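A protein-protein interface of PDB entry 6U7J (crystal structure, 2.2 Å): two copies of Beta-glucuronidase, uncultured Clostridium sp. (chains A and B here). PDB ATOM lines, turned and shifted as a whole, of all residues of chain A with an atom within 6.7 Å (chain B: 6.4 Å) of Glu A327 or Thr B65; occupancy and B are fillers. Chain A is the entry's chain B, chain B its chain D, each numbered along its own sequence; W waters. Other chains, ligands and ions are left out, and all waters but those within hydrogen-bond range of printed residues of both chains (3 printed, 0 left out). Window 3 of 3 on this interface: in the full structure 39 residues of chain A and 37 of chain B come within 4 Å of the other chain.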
ATOM      1  N   ASN A 322     -16.395 -13.528  -8.709  1.00  0.00           N
ATOM      2  CA  ASN A 322     -15.645 -14.669  -8.190  1.00  0.00           C
ATOM      3  C   ASN A 322     -14.712 -15.247  -9.245  1.00  0.00           C
ATOM      4  O   ASN A 322     -13.580 -15.632  -8.937  1.00  0.00           O
ATOM      5  CB  ASN A 322     -16.601 -15.755  -7.691  1.00  0.00           C
ATOM      6  CG  ASN A 322     -17.384 -15.319  -6.466  1.00  0.00           C
ATOM      7  OD1 ASN A 322     -17.027 -14.337  -5.805  1.00  0.00           O
ATOM      8  ND2 ASN A 322     -18.465 -16.029  -6.168  1.00  0.00           N
ATOM      9  N   VAL A 323     -15.179 -15.354 -10.488  1.00  0.00           N
ATOM     10  CA  VAL A 323     -14.325 -15.932 -11.519  1.00  0.00           C
ATOM     11  C   VAL A 323     -13.144 -15.017 -11.782  1.00  0.00           C
ATOM     12  O   VAL A 323     -12.002 -15.469 -11.900  1.00  0.00           O
ATOM     13  CB  VAL A 323     -15.117 -16.207 -12.808  1.00  0.00           C
ATOM     14  CG1 VAL A 323     -14.160 -16.670 -13.904  1.00  0.00           C
ATOM     15  CG2 VAL A 323     -16.228 -17.247 -12.568  1.00  0.00           C
ATOM     16  N   ARG A 324     -13.395 -13.711 -11.845  1.00  0.00           N
ATOM     17  CA  ARG A 324     -12.303 -12.757 -12.006  1.00  0.00           C
ATOM     18  C   ARG A 324     -11.317 -12.870 -10.854  1.00  0.00           C
ATOM     19  O   ARG A 324     -10.100 -12.831 -11.068  1.00  0.00           O
ATOM     20  CB  ARG A 324     -12.880 -11.337 -12.129  1.00  0.00           C
ATOM     21  CG  ARG A 324     -11.880 -10.200 -11.964  1.00  0.00           C
ATOM     22  CD  ARG A 324     -10.986 -10.060 -13.191  1.00  0.00           C
ATOM     23  NE  ARG A 324     -10.072  -8.924 -13.065  1.00  0.00           N
ATOM     24  CZ  ARG A 324      -9.144  -8.598 -13.958  1.00  0.00           C
ATOM     25  NH1 ARG A 324      -8.985  -9.325 -15.052  1.00  0.00           N
ATOM     26  NH2 ARG A 324      -8.368  -7.543 -13.749  1.00  0.00           N
ATOM     27  N   ASP A 325     -11.820 -13.055  -9.624  1.00  0.00           N
ATOM     28  CA  ASP A 325     -10.925 -13.195  -8.469  1.00  0.00           C
ATOM     29  C   ASP A 325     -10.062 -14.454  -8.581  1.00  0.00           C
ATOM     30  O   ASP A 325      -8.859 -14.419  -8.289  1.00  0.00           O
ATOM     31  CB  ASP A 325     -11.730 -13.208  -7.164  1.00  0.00           C
ATOM     32  CG  ASP A 325     -12.230 -11.808  -6.748  1.00  0.00           C
ATOM     33  OD1 ASP A 325     -12.057 -10.842  -7.523  1.00  0.00           O
ATOM     34  OD2 ASP A 325     -12.804 -11.669  -5.638  1.00  0.00           O
ATOM     35  N   CYS A 326     -10.647 -15.577  -9.022  1.00  0.00           N
ATOM     36  CA  CYS A 326      -9.848 -16.791  -9.171  1.00  0.00           C
ATOM     37  C   CYS A 326      -8.836 -16.648 -10.301  1.00  0.00           C
ATOM     38  O   CYS A 326      -7.727 -17.200 -10.222  1.00  0.00           O
ATOM     39  CB  CYS A 326     -10.745 -17.991  -9.437  1.00  0.00           C
ATOM     40  SG  CYS A 326     -11.820 -18.376  -8.049  1.00  0.00           S
ATOM     41  N   GLU A 327      -9.192 -15.909 -11.357  1.00  0.00           N
ATOM     42  CA  GLU A 327      -8.224 -15.590 -12.409  1.00  0.00           C
ATOM     43  C   GLU A 327      -7.058 -14.783 -11.851  1.00  0.00           C
ATOM     44  O   GLU A 327      -5.905 -14.968 -12.263  1.00  0.00           O
ATOM     45  CB  GLU A 327      -8.909 -14.817 -13.541  1.00  0.00           C
ATOM     46  CG  GLU A 327      -9.827 -15.649 -14.438  1.00  0.00           C
ATOM     47  CD  GLU A 327      -9.036 -16.489 -15.446  1.00  0.00           C
ATOM     48  OE1 GLU A 327      -7.953 -16.037 -15.887  1.00  0.00           O
ATOM     49  OE2 GLU A 327      -9.491 -17.600 -15.794  1.00  0.00           O
ATOM     50  N   LEU A 328      -7.338 -13.874 -10.919  1.00  0.00           N
ATOM     51  CA  LEU A 328      -6.270 -13.044 -10.372  1.00  0.00           C
ATOM     52  C   LEU A 328      -5.410 -13.841  -9.403  1.00  0.00           C
ATOM     53  O   LEU A 328      -4.180 -13.689  -9.380  1.00  0.00           O
ATOM     54  CB  LEU A 328      -6.861 -11.811  -9.689  1.00  0.00           C
ATOM     55  CG  LEU A 328      -7.532 -10.739 -10.566  1.00  0.00           C
ATOM     56  CD1 LEU A 328      -8.182  -9.669  -9.694  1.00  0.00           C
ATOM     57  CD2 LEU A 328      -6.528 -10.090 -11.506  1.00  0.00           C
ATOM     58  N   LEU A 329      -6.046 -14.690  -8.589  1.00  0.00           N
ATOM     59  CA  LEU A 329      -5.305 -15.600  -7.723  1.00  0.00           C
ATOM     60  C   LEU A 329      -4.339 -16.450  -8.533  1.00  0.00           C
ATOM     61  O   LEU A 329      -3.173 -16.615  -8.164  1.00  0.00           O
ATOM     62  CB  LEU A 329      -6.270 -16.501  -6.950  1.00  0.00           C
ATOM     63  CG  LEU A 329      -7.056 -15.846  -5.822  1.00  0.00           C
ATOM     64  CD1 LEU A 329      -8.090 -16.821  -5.271  1.00  0.00           C
ATOM     65  CD2 LEU A 329      -6.127 -15.344  -4.714  1.00  0.00           C
ATOM     66  N   LYS A 330      -4.815 -16.999  -9.647  1.00  0.00           N
ATOM     67  CA  LYS A 330      -3.951 -17.811 -10.491  1.00  0.00           C
ATOM     68  C   LYS A 330      -2.844 -16.969 -11.114  1.00  0.00           C
ATOM     69  O   LYS A 330      -1.696 -17.415 -11.212  1.00  0.00           O
ATOM     70  CB  LYS A 330      -4.787 -18.494 -11.571  1.00  0.00           C
ATOM     71  CG  LYS A 330      -3.972 -19.374 -12.517  1.00  0.00           C
ATOM     72  CD  LYS A 330      -4.832 -19.793 -13.702  1.00  0.00           C
ATOM     73  CE  LYS A 330      -4.142 -20.843 -14.542  1.00  0.00           C
ATOM     74  NZ  LYS A 330      -3.897 -22.084 -13.740  1.00  0.00           N
ATOM     75  N   TRP A 331      -3.168 -15.748 -11.540  1.00  0.00           N
ATOM     76  CA  TRP A 331      -2.172 -14.900 -12.188  1.00  0.00           C
ATOM     77  C   TRP A 331      -1.068 -14.522 -11.213  1.00  0.00           C
ATOM     78  O   TRP A 331       0.117 -14.606 -11.544  1.00  0.00           O
ATOM     79  CB  TRP A 331      -2.850 -13.653 -12.765  1.00  0.00           C
ATOM     80  CG  TRP A 331      -1.893 -12.589 -13.268  1.00  0.00           C
ATOM     81  CD1 TRP A 331      -1.314 -12.511 -14.512  1.00  0.00           C
ATOM     82  CD2 TRP A 331      -1.435 -11.446 -12.544  1.00  0.00           C
ATOM     83  NE1 TRP A 331      -0.521 -11.392 -14.599  1.00  0.00           N
ATOM     84  CE2 TRP A 331      -0.574 -10.721 -13.405  1.00  0.00           C
ATOM     85  CE3 TRP A 331      -1.672 -10.958 -11.253  1.00  0.00           C
ATOM     86  CZ2 TRP A 331       0.058  -9.544 -13.009  1.00  0.00           C
ATOM     87  CZ3 TRP A 331      -1.038  -9.786 -10.857  1.00  0.00           C
ATOM     88  CH2 TRP A 331      -0.184  -9.091 -11.737  1.00  0.00           C
ATOM     89  N   ILE A 332      -1.435 -14.150  -9.987  1.00  0.00           N
ATOM     90  CA  ILE A 332      -0.438 -13.717  -9.016  1.00  0.00           C
ATOM     91  C   ILE A 332       0.341 -14.875  -8.417  1.00  0.00           C
ATOM     92  O   ILE A 332       1.315 -14.633  -7.698  1.00  0.00           O
ATOM     93  CB  ILE A 332      -1.102 -12.889  -7.899  1.00  0.00           C
ATOM     94  CG1 ILE A 332      -0.086 -11.919  -7.270  1.00  0.00           C
ATOM     95  CG2 ILE A 332      -1.763 -13.805  -6.885  1.00  0.00           C
ATOM     96  CD1 ILE A 332      -0.693 -10.752  -6.508  1.00  0.00           C
ATOM     97  N   LYS A 355     -11.098 -25.700  -8.919  1.00  0.00           N
ATOM     98  CA  LYS A 355      -9.825 -25.150  -9.360  1.00  0.00           C
ATOM     99  C   LYS A 355      -8.650 -25.616  -8.515  1.00  0.00           C
ATOM    100  O   LYS A 355      -7.515 -25.231  -8.801  1.00  0.00           O
ATOM    101  CB  LYS A 355      -9.881 -23.623  -9.367  1.00  0.00           C
ATOM    102  CG  LYS A 355     -10.781 -23.055 -10.440  1.00  0.00           C
ATOM    103  CD  LYS A 355     -10.950 -21.559 -10.232  1.00  0.00           C
ATOM    104  CE  LYS A 355     -11.971 -20.986 -11.196  1.00  0.00           C
ATOM    105  NZ  LYS A 355     -11.691 -21.376 -12.599  1.00  0.00           N
ATOM    106  N   ILE B  53     -11.931 -23.288 -19.480  1.00  0.00           N
ATOM    107  CA  ILE B  53     -11.856 -22.517 -18.252  1.00  0.00           C
ATOM    108  C   ILE B  53     -13.286 -22.186 -17.839  1.00  0.00           C
ATOM    109  O   ILE B  53     -14.233 -22.427 -18.582  1.00  0.00           O
ATOM    110  CB  ILE B  53     -11.023 -21.232 -18.421  1.00  0.00           C
ATOM    111  CG1 ILE B  53     -11.688 -20.317 -19.463  1.00  0.00           C
ATOM    112  CG2 ILE B  53      -9.576 -21.574 -18.799  1.00  0.00           C
ATOM    113  CD1 ILE B  53     -11.004 -18.978 -19.673  1.00  0.00           C
ATOM    114  N   ASP B  54     -13.432 -21.625 -16.644  1.00  0.00           N
ATOM    115  CA  ASP B  54     -14.734 -21.172 -16.169  1.00  0.00           C
ATOM    116  C   ASP B  54     -15.091 -19.805 -16.738  1.00  0.00           C
ATOM    117  O   ASP B  54     -14.236 -18.923 -16.878  1.00  0.00           O
ATOM    118  CB  ASP B  54     -14.753 -21.107 -14.647  1.00  0.00           C
ATOM    119  CG  ASP B  54     -14.653 -22.483 -14.008  1.00  0.00           C
ATOM    120  OD1 ASP B  54     -15.152 -23.470 -14.600  1.00  0.00           O
ATOM    121  OD2 ASP B  54     -14.055 -22.577 -12.914  1.00  0.00           O
ATOM    122  N   MET B  55     -16.373 -19.627 -17.079  1.00  0.00           N
ATOM    123  CA  MET B  55     -16.843 -18.348 -17.582  1.00  0.00           C
ATOM    124  C   MET B  55     -18.228 -18.109 -16.997  1.00  0.00           C
ATOM    125  O   MET B  55     -19.106 -18.973 -17.126  1.00  0.00           O
ATOM    126  CB  MET B  55     -16.888 -18.296 -19.111  1.00  0.00           C
ATOM    127  CG  MET B  55     -17.126 -16.885 -19.675  1.00  0.00           C
ATOM    128  SD  MET B  55     -15.761 -15.754 -19.298  1.00  0.00           S
ATOM    129  CE  MET B  55     -14.314 -16.605 -19.939  1.00  0.00           C
ATOM    130  N   TYR B  61     -17.111 -12.051 -22.008  1.00  0.00           N
ATOM    131  CA  TYR B  61     -15.923 -12.795 -21.602  1.00  0.00           C
ATOM    132  C   TYR B  61     -14.652 -11.945 -21.607  1.00  0.00           C
ATOM    133  O   TYR B  61     -13.642 -12.372 -21.040  1.00  0.00           O
ATOM    134  CB  TYR B  61     -15.727 -14.050 -22.484  1.00  0.00           C
ATOM    135  CG  TYR B  61     -15.504 -13.801 -23.963  1.00  0.00           C
ATOM    136  CD1 TYR B  61     -14.285 -13.335 -24.448  1.00  0.00           C
ATOM    137  CD2 TYR B  61     -16.511 -14.072 -24.883  1.00  0.00           C
ATOM    138  CE1 TYR B  61     -14.085 -13.120 -25.821  1.00  0.00           C
ATOM    139  CE2 TYR B  61     -16.326 -13.858 -26.237  1.00  0.00           C
ATOM    140  CZ  TYR B  61     -15.118 -13.387 -26.707  1.00  0.00           C
ATOM    141  OH  TYR B  61     -14.964 -13.202 -28.072  1.00  0.00           O
ATOM    142  N   ASN B  62     -14.695 -10.734 -22.166  1.00  0.00           N
ATOM    143  CA  ASN B  62     -13.460 -10.030 -22.522  1.00  0.00           C
ATOM    144  C   ASN B  62     -12.686  -9.514 -21.313  1.00  0.00           C
ATOM    145  O   ASN B  62     -11.457  -9.382 -21.396  1.00  0.00           O
ATOM    146  CB  ASN B  62     -13.760  -8.860 -23.461  1.00  0.00           C
ATOM    147  CG  ASN B  62     -14.628  -9.268 -24.634  1.00  0.00           C
ATOM    148  OD1 ASN B  62     -15.837  -9.493 -24.481  1.00  0.00           O
ATOM    149  ND2 ASN B  62     -14.019  -9.360 -25.819  1.00  0.00           N
ATOM    150  N   ASP B  63     -13.362  -9.180 -20.210  1.00  0.00           N
ATOM    151  CA  ASP B  63     -12.704  -8.553 -19.063  1.00  0.00           C
ATOM    152  C   ASP B  63     -12.583  -9.481 -17.862  1.00  0.00           C
ATOM    153  O   ASP B  63     -12.201  -9.025 -16.772  1.00  0.00           O
ATOM    154  CB  ASP B  63     -13.448  -7.281 -18.646  1.00  0.00           C
ATOM    155  CG  ASP B  63     -13.170  -6.116 -19.567  1.00  0.00           C
ATOM    156  OD1 ASP B  63     -12.298  -6.264 -20.456  1.00  0.00           O
ATOM    157  OD2 ASP B  63     -13.830  -5.058 -19.402  1.00  0.00           O
ATOM    158  N   ILE B  64     -12.886 -10.767 -18.035  1.00  0.00           N
ATOM    159  CA  ILE B  64     -12.853 -11.711 -16.925  1.00  0.00           C
ATOM    160  C   ILE B  64     -11.434 -12.225 -16.677  1.00  0.00           C
ATOM    161  O   ILE B  64     -11.024 -12.400 -15.525  1.00  0.00           O
ATOM    162  CB  ILE B  64     -13.838 -12.874 -17.190  1.00  0.00           C
ATOM    163  CG1 ILE B  64     -15.295 -12.371 -17.223  1.00  0.00           C
ATOM    164  CG2 ILE B  64     -13.657 -13.977 -16.143  1.00  0.00           C
ATOM    165  CD1 ILE B  64     -15.793 -11.861 -15.875  1.00  0.00           C
ATOM    166  N   THR B  65     -10.658 -12.488 -17.725  1.00  0.00           N
ATOM    167  CA  THR B  65      -9.360 -13.120 -17.514  1.00  0.00           C
ATOM    168  C   THR B  65      -8.247 -12.084 -17.554  1.00  0.00           C
ATOM    169  O   THR B  65      -8.459 -10.918 -17.879  1.00  0.00           O
ATOM    170  CB  THR B  65      -9.075 -14.213 -18.553  1.00  0.00           C
ATOM    171  OG1 THR B  65      -8.791 -13.603 -19.816  1.00  0.00           O
ATOM    172  CG2 THR B  65     -10.265 -15.197 -18.691  1.00  0.00           C
ATOM    173  N   THR B  66      -7.033 -12.548 -17.253  1.00  0.00           N
ATOM    174  CA  THR B  66      -5.833 -11.732 -17.300  1.00  0.00           C
ATOM    175  C   THR B  66      -5.147 -11.792 -18.661  1.00  0.00           C
ATOM    176  O   THR B  66      -4.006 -11.349 -18.798  1.00  0.00           O
ATOM    177  CB  THR B  66      -4.876 -12.173 -16.188  1.00  0.00           C
ATOM    178  OG1 THR B  66      -4.472 -13.532 -16.413  1.00  0.00           O
ATOM    179  CG2 THR B  66      -5.575 -12.075 -14.831  1.00  0.00           C
ATOM    180  N   ASP B  67      -5.844 -12.273 -19.673  1.00  0.00           N
ATOM    181  CA  ASP B  67      -5.257 -12.719 -20.928  1.00  0.00           C
ATOM    182  C   ASP B  67      -5.619 -11.739 -22.047  1.00  0.00           C
ATOM    183  O   ASP B  67      -6.771 -11.697 -22.493  1.00  0.00           O
ATOM    184  CB  ASP B  67      -5.774 -14.131 -21.227  1.00  0.00           C
ATOM    185  CG  ASP B  67      -5.290 -14.660 -22.542  1.00  0.00           C
ATOM    186  OD1 ASP B  67      -5.948 -15.562 -23.101  1.00  0.00           O
ATOM    187  OD2 ASP B  67      -4.241 -14.176 -23.015  1.00  0.00           O
ATOM    188  N   GLN B  68      -4.631 -10.981 -22.531  1.00  0.00           N
ATOM    189  CA  GLN B  68      -4.901 -10.042 -23.621  1.00  0.00           C
ATOM    190  C   GLN B  68      -5.408 -10.748 -24.878  1.00  0.00           C
ATOM    191  O   GLN B  68      -6.205 -10.175 -25.620  1.00  0.00           O
ATOM    192  CB  GLN B  68      -3.650  -9.203 -23.941  1.00  0.00           C
ATOM    193  CG  GLN B  68      -2.836  -9.670 -25.162  1.00  0.00           C
ATOM    194  CD  GLN B  68      -1.677  -8.734 -25.489  1.00  0.00           C
ATOM    195  OE1 GLN B  68      -1.835  -7.510 -25.462  1.00  0.00           O
ATOM    196  NE2 GLN B  68      -0.496  -9.306 -25.782  1.00  0.00           N
ATOM    197  N   LEU B  70      -7.451 -13.334 -25.121  1.00  0.00           N
ATOM    198  CA  LEU B  70      -8.891 -13.537 -25.033  1.00  0.00           C
ATOM    199  C   LEU B  70      -9.627 -12.200 -25.107  1.00  0.00           C
ATOM    200  O   LEU B  70     -10.632 -12.082 -25.812  1.00  0.00           O
ATOM    201  CB  LEU B  70      -9.243 -14.296 -23.753  1.00  0.00           C
ATOM    202  CG  LEU B  70     -10.744 -14.585 -23.577  1.00  0.00           C
ATOM    203  CD1 LEU B  70     -11.286 -15.397 -24.746  1.00  0.00           C
ATOM    204  CD2 LEU B  70     -11.059 -15.278 -22.249  1.00  0.00           C
ATOM    205  N   ARG B  71      -9.117 -11.176 -24.416  1.00  0.00           N
ATOM    206  CA  ARG B  71      -9.771  -9.865 -24.432  1.00  0.00           C
ATOM    207  C   ARG B  71      -9.989  -9.381 -25.860  1.00  0.00           C
ATOM    208  O   ARG B  71     -11.099  -8.975 -26.233  1.00  0.00           O
ATOM    209  CB  ARG B  71      -8.934  -8.845 -23.643  1.00  0.00           C
ATOM    210  CG  ARG B  71      -9.543  -7.419 -23.575  1.00  0.00           C
ATOM    211  CD  ARG B  71      -8.521  -6.408 -23.081  1.00  0.00           C
ATOM    212  NE  ARG B  71      -7.476  -6.193 -24.078  1.00  0.00           N
ATOM    213  CZ  ARG B  71      -6.296  -5.628 -23.832  1.00  0.00           C
ATOM    214  NH1 ARG B  71      -5.980  -5.214 -22.604  1.00  0.00           N
ATOM    215  NH2 ARG B  71      -5.432  -5.471 -24.823  1.00  0.00           N
HETATM  216  O   HOH W   1     -11.072 -22.322 -14.784  1.00  0.00           O
HETATM  217  O   HOH W   2      -5.291 -15.847 -14.807  1.00  0.00           O
HETATM  218  O   HOH W   3     -11.770 -18.642 -15.599  1.00  0.00           O
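No position is printed for both chains.
Of the 11 pairs that touch across the chains among the printed residues, none has its exchanged pair printed and touching as well.
Of the printed residues of chain B, Arg A324 touches Asp B63, Ile B64 and Thr B65.
Of the printed residues of chain B, Leu A328 touches Thr B66 (3.99 Å).
Lys A330 touches none of the printed residues of chain B.
Of the printed residues of chain B, Trp A331 touches Thr B66.
Of the printed residues of chain B, Lys A355 touches Asp B54.
Of chain A, only Arg A324 and Glu A327 come within 4 Å of Thr B65.
Printed residues of chain A within 4 Å of Thr B66: Glu A327, Leu A328 and Trp A331.
Leu B70 touches none of the printed residues of chain A.
The nearest residue of chain A that does not touch Thr B65 is Val A323 (6.3 Å).
Water W1 lies within hydrogen-bond range of the side-chain amino group (NZ) of Lys A355 (2.5 Å) and the backbone NH (N) of Asp B54 (3.1 Å).
Water W3 bridges OE2 of Glu A327 (2.5 Å) and O of Asp B54 (2.8 Å).
Water W2 lies within hydrogen-bond range of the backbone carbonyl oxygen of Glu A327 and the side-chain hydroxyl of Thr B66.
Of the 12 printed residues of chain A, 6 touch a printed residue of chain B.
Hydrophobic or aromatic side chains of chain A that line the printed part of chain B: Val A323, Leu A328 and Trp A331.
Hydrophobic or aromatic side chains of chain B that line the printed part of chain A: Ile B64.
Among the printed residues, 11 pairs touch across the chains.
N of Asp B67 sits close to OG1 of Thr B65 (3.2 Å).
Val A323 touches Asp B54 (CG1 to O, 3.7 Å).
Ile B64 touches Val A323.
NH1 of Arg A324 touches O of Asp B63, at 3.7 Å.
Arg A324 touches Ile B64 (CD to O, 3.3 Å).
Ile B64 touches Glu A327.
Glu A327 touches Thr B65.
Glu A327 touches Thr B66.
Leu A328 touches Thr B66 (CD2 to CG2, 3.99 Å).
Trp A331 touches Thr B66.
NZ of Lys A355 lies within salt-bridge range of OD2 of Asp B54, at 2.7 Å.
The guanidinium group of Arg A324 is in hydrogen-bond range of the backbone carbonyl oxygen of Thr B65 (3.3 Å).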
